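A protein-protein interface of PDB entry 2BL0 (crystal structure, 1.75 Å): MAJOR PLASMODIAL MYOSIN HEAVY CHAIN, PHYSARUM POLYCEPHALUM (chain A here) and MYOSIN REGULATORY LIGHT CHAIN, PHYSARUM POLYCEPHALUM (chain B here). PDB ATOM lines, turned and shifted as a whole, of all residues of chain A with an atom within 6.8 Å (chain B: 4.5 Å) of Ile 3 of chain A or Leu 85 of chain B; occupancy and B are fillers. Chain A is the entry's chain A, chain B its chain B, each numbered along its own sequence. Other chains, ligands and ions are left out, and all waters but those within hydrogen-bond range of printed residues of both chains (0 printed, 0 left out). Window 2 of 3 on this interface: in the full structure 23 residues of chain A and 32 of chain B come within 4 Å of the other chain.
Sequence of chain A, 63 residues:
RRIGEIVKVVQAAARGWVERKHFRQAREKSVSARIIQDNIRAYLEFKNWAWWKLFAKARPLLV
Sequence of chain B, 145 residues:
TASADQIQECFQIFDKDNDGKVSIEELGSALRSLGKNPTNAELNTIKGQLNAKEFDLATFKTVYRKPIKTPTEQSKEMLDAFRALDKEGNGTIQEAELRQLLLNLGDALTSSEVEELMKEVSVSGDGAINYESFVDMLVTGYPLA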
ATOM      1  N   ARG A   1     -19.289  20.703 -30.950  1.00  0.00           N
ATOM      2  CA  ARG A   1     -18.576  21.424 -32.051  1.00  0.00           C
ATOM      3  C   ARG A   1     -17.989  22.731 -31.546  1.00  0.00           C
ATOM      4  O   ARG A   1     -17.035  22.723 -30.772  1.00  0.00           O
ATOM      5  N   ARG A   2     -18.555  23.856 -31.979  1.00  0.00           N
ATOM      6  CA  ARG A   2     -18.243  25.143 -31.371  1.00  0.00           C
ATOM      7  C   ARG A   2     -18.879  25.212 -29.969  1.00  0.00           C
ATOM      8  O   ARG A   2     -18.363  25.893 -29.087  1.00  0.00           O
ATOM      9  CB  ARG A   2     -18.685  26.319 -32.257  1.00  0.00           C
ATOM     10  CG  ARG A   2     -17.760  27.576 -32.129  1.00  0.00           C
ATOM     11  CD  ARG A   2     -17.028  28.073 -33.414  1.00  0.00           C
ATOM     12  NE  ARG A   2     -16.881  27.093 -34.496  1.00  0.00           N
ATOM     13  CZ  ARG A   2     -16.058  26.041 -34.485  1.00  0.00           C
ATOM     14  NH1 ARG A   2     -16.023  25.225 -35.536  1.00  0.00           N
ATOM     15  NH2 ARG A   2     -15.281  25.786 -33.436  1.00  0.00           N
ATOM     16  N   ILE A   3     -19.974  24.474 -29.769  1.00  0.00           N
ATOM     17  CA  ILE A   3     -20.656  24.397 -28.469  1.00  0.00           C
ATOM     18  C   ILE A   3     -19.789  23.718 -27.409  1.00  0.00           C
ATOM     19  O   ILE A   3     -19.730  24.182 -26.280  1.00  0.00           O
ATOM     20  CB  ILE A   3     -21.998  23.628 -28.579  1.00  0.00           C
ATOM     21  CG1 ILE A   3     -22.954  24.310 -29.565  1.00  0.00           C
ATOM     22  CG2 ILE A   3     -22.670  23.505 -27.202  1.00  0.00           C
ATOM     23  CD1 ILE A   3     -23.288  25.738 -29.218  1.00  0.00           C
ATOM     24  N   GLY A   4     -19.156  22.607 -27.775  1.00  0.00           N
ATOM     25  CA  GLY A   4     -18.173  21.966 -26.924  1.00  0.00           C
ATOM     26  C   GLY A   4     -17.124  22.949 -26.430  1.00  0.00           C
ATOM     27  O   GLY A   4     -16.724  22.904 -25.268  1.00  0.00           O
ATOM     28  N   GLU A   5     -16.689  23.862 -27.294  1.00  0.00           N
ATOM     29  CA  GLU A   5     -15.646  24.816 -26.895  1.00  0.00           C
ATOM     30  C   GLU A   5     -16.190  25.905 -25.976  1.00  0.00           C
ATOM     31  O   GLU A   5     -15.573  26.191 -24.958  1.00  0.00           O
ATOM     32  CB  GLU A   5     -14.932  25.455 -28.103  1.00  0.00           C
ATOM     33  CG  GLU A   5     -13.622  24.774 -28.529  1.00  0.00           C
ATOM     34  CD  GLU A   5     -12.654  24.485 -27.390  1.00  0.00           C
ATOM     35  OE1 GLU A   5     -12.333  23.294 -27.187  1.00  0.00           O
ATOM     36  OE2 GLU A   5     -12.195  25.433 -26.710  1.00  0.00           O
ATOM     37  N   ILE A   6     -17.355  26.479 -26.288  1.00  0.00           N
ATOM     38  CA  ILE A   6     -17.838  27.638 -25.528  1.00  0.00           C
ATOM     39  C   ILE A   6     -18.263  27.263 -24.117  1.00  0.00           C
ATOM     40  O   ILE A   6     -18.246  28.121 -23.238  1.00  0.00           O
ATOM     41  CB  ILE A   6     -18.993  28.411 -26.249  1.00  0.00           C
ATOM     42  CG1 ILE A   6     -20.326  27.649 -26.153  1.00  0.00           C
ATOM     43  CG2 ILE A   6     -18.614  28.743 -27.707  1.00  0.00           C
ATOM     44  CD1 ILE A   6     -21.464  28.290 -26.945  1.00  0.00           C
ATOM     45  N   VAL A   7     -18.672  26.008 -23.900  1.00  0.00           N
ATOM     46  CA  VAL A   7     -19.144  25.608 -22.565  1.00  0.00           C
ATOM     47  C   VAL A   7     -18.012  25.268 -21.608  1.00  0.00           C
ATOM     48  O   VAL A   7     -18.239  25.157 -20.410  1.00  0.00           O
ATOM     49  CB  VAL A   7     -20.162  24.444 -22.567  1.00  0.00           C
ATOM     50  CG1 VAL A   7     -21.435  24.847 -23.347  1.00  0.00           C
ATOM     51  CG2 VAL A   7     -19.547  23.132 -23.054  1.00  0.00           C
ATOM     52  N   LYS A   8     -16.803  25.074 -22.130  1.00  0.00           N
ATOM     53  CA  LYS A   8     -15.668  24.767 -21.253  1.00  0.00           C
ATOM     54  C   LYS A   8     -15.479  25.814 -20.149  1.00  0.00           C
ATOM     55  O   LYS A   8     -15.126  25.455 -19.037  1.00  0.00           O
ATOM     56  CB  LYS A   8     -14.368  24.594 -22.051  1.00  0.00           C
ATOM     57  CG  LYS A   8     -14.255  23.235 -22.755  1.00  0.00           C
ATOM     58  CD  LYS A   8     -13.060  23.174 -23.708  1.00  0.00           C
ATOM     59  CE  LYS A   8     -13.069  21.881 -24.528  1.00  0.00           C
ATOM     60  NZ  LYS A   8     -11.849  21.760 -25.403  1.00  0.00           N
ATOM     61  N   VAL A  10     -17.843  27.584 -18.740  1.00  0.00           N
ATOM     62  CA  VAL A  10     -18.937  27.316 -17.796  1.00  0.00           C
ATOM     63  C   VAL A  10     -18.577  26.088 -16.959  1.00  0.00           C
ATOM     64  O   VAL A  10     -18.758  26.090 -15.761  1.00  0.00           O
ATOM     65  CB  VAL A  10     -20.304  27.105 -18.491  1.00  0.00           C
ATOM     66  CG1 VAL A  10     -21.410  26.906 -17.451  1.00  0.00           C
ATOM     67  CG2 VAL A  10     -20.668  28.302 -19.400  1.00  0.00           C
ATOM     68  N   ALA B  81     -21.482  32.899 -23.843  1.00  0.00           N
ATOM     69  CA  ALA B  81     -21.812  31.504 -24.136  1.00  0.00           C
ATOM     70  C   ALA B  81     -23.304  31.283 -23.997  1.00  0.00           C
ATOM     71  O   ALA B  81     -23.926  30.753 -24.888  1.00  0.00           O
ATOM     72  CB  ALA B  81     -21.064  30.565 -23.221  1.00  0.00           C
ATOM     73  N   PHE B  82     -23.889  31.705 -22.876  1.00  0.00           N
ATOM     74  CA  PHE B  82     -25.308  31.461 -22.642  1.00  0.00           C
ATOM     75  C   PHE B  82     -26.186  32.261 -23.598  1.00  0.00           C
ATOM     76  O   PHE B  82     -27.216  31.792 -24.041  1.00  0.00           O
ATOM     77  CB  PHE B  82     -25.702  31.749 -21.184  1.00  0.00           C
ATOM     78  CG  PHE B  82     -25.391  30.620 -20.235  1.00  0.00           C
ATOM     79  CD1 PHE B  82     -25.990  29.378 -20.385  1.00  0.00           C
ATOM     80  CD2 PHE B  82     -24.495  30.791 -19.193  1.00  0.00           C
ATOM     81  CE1 PHE B  82     -25.706  28.343 -19.523  1.00  0.00           C
ATOM     82  CE2 PHE B  82     -24.209  29.756 -18.318  1.00  0.00           C
ATOM     83  CZ  PHE B  82     -24.804  28.521 -18.490  1.00  0.00           C
ATOM     84  N   ARG B  83     -25.774  33.472 -23.929  1.00  0.00           N
ATOM     85  CA  ARG B  83     -26.528  34.273 -24.886  1.00  0.00           C
ATOM     86  C   ARG B  83     -26.600  33.577 -26.251  1.00  0.00           C
ATOM     87  O   ARG B  83     -27.615  33.655 -26.939  1.00  0.00           O
ATOM     88  CB  ARG B  83     -25.884  35.639 -25.044  1.00  0.00           C
ATOM     89  CG  ARG B  83     -26.656  36.572 -25.971  1.00  0.00           C
ATOM     90  CD  ARG B  83     -28.066  36.861 -25.513  1.00  0.00           C
ATOM     91  NE  ARG B  83     -28.448  38.190 -25.973  1.00  0.00           N
ATOM     92  CZ  ARG B  83     -29.296  38.461 -26.952  1.00  0.00           C
ATOM     93  NH1 ARG B  83     -29.929  37.484 -27.612  1.00  0.00           N
ATOM     94  NH2 ARG B  83     -29.516  39.742 -27.271  1.00  0.00           N
ATOM     95  N   ALA B  84     -25.515  32.912 -26.624  1.00  0.00           N
ATOM     96  CA  ALA B  84     -25.431  32.200 -27.895  1.00  0.00           C
ATOM     97  C   ALA B  84     -26.313  30.954 -27.903  1.00  0.00           C
ATOM     98  O   ALA B  84     -26.647  30.431 -28.976  1.00  0.00           O
ATOM     99  CB  ALA B  84     -23.986  31.813 -28.166  1.00  0.00           C
ATOM    100  N   LEU B  85     -26.654  30.466 -26.708  1.00  0.00           N
ATOM    101  CA  LEU B  85     -27.549  29.325 -26.518  1.00  0.00           C
ATOM    102  C   LEU B  85     -29.003  29.739 -26.257  1.00  0.00           C
ATOM    103  O   LEU B  85     -29.898  28.892 -26.242  1.00  0.00           O
ATOM    104  CB  LEU B  85     -27.029  28.455 -25.372  1.00  0.00           C
ATOM    105  CG  LEU B  85     -25.601  27.920 -25.576  1.00  0.00           C
ATOM    106  CD1 LEU B  85     -25.009  27.314 -24.314  1.00  0.00           C
ATOM    107  CD2 LEU B  85     -25.590  26.920 -26.715  1.00  0.00           C
ATOM    108  N   ASP B  86     -29.247  31.042 -26.121  1.00  0.00           N
ATOM    109  CA  ASP B  86     -30.556  31.572 -25.736  1.00  0.00           C
ATOM    110  C   ASP B  86     -31.472  31.715 -26.960  1.00  0.00           C
ATOM    111  O   ASP B  86     -31.373  32.695 -27.696  1.00  0.00           O
ATOM    112  CB  ASP B  86     -30.350  32.921 -25.027  1.00  0.00           C
ATOM    113  CG  ASP B  86     -31.635  33.541 -24.538  1.00  0.00           C
ATOM    114  OD1 ASP B  86     -32.731  33.044 -24.894  1.00  0.00           O
ATOM    115  OD2 ASP B  86     -31.633  34.559 -23.800  1.00  0.00           O
ATOM    116  N   LYS B  87     -32.363  30.741 -27.159  1.00  0.00           N
ATOM    117  CA  LYS B  87     -33.240  30.698 -28.337  1.00  0.00           C
ATOM    118  C   LYS B  87     -34.336  31.759 -28.376  1.00  0.00           C
ATOM    119  O   LYS B  87     -34.716  32.226 -29.455  1.00  0.00           O
ATOM    120  CB  LYS B  87     -33.920  29.317 -28.469  1.00  0.00           C
ATOM    121  CG  LYS B  87     -33.031  28.098 -28.316  1.00  0.00           C
ATOM    122  CD  LYS B  87     -33.839  26.823 -28.647  1.00  0.00           C
ATOM    123  CE  LYS B  87     -32.977  25.573 -28.684  1.00  0.00           C
ATOM    124  NZ  LYS B  87     -33.685  24.454 -29.391  1.00  0.00           N
ATOM    125  N   LEU B 101     -25.344  19.686 -21.870  1.00  0.00           N
ATOM    126  CA  LEU B 101     -24.121  20.329 -22.334  1.00  0.00           C
ATOM    127  C   LEU B 101     -23.002  20.081 -21.338  1.00  0.00           C
ATOM    128  O   LEU B 101     -21.920  19.643 -21.736  1.00  0.00           O
ATOM    129  CB  LEU B 101     -24.353  21.821 -22.543  1.00  0.00           C
ATOM    130  CG  LEU B 101     -25.335  22.144 -23.681  1.00  0.00           C
ATOM    131  CD1 LEU B 101     -25.523  23.645 -23.783  1.00  0.00           C
ATOM    132  CD2 LEU B 101     -24.884  21.543 -25.026  1.00  0.00           C
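Ile 3 of chain A touches two residues of chain B. Leu 85 of chain B touches one residue of chain A. Printed residues of chain A within 4 Å of Phe 82 of chain B: Val 10. Of the printed residues of chain B, Val 10 of chain A touches Phe 82. Glu 5 of chain A touches none of the printed residues of chain B.
Printed residues of chain A that touch a printed residue of chain B: Ile 3, Ile 6 and Val 10. Hydrophobic or aromatic side chains of chain A within 4 Å of the printed part of chain B: Ile 3 and Val 10. Among the printed residues, 4 pairs touch across the chains. Among the printed residues, no Asp or Glu carboxylate lies within 4 Å of a Lys or Arg side-chain nitrogen of the other chain.
Among the printed residues, merely in contact across the chains: Ile 3 of chain A with Leu 85 of chain B (3.6 Å), Ile 3 of chain A with Leu 101 of chain B (3.7 Å), Ile 6 of chain A with Ala 81 of chain B (3.7 Å) and Val 10 of chain A with Phe 82 of chain B (3.9 Å).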
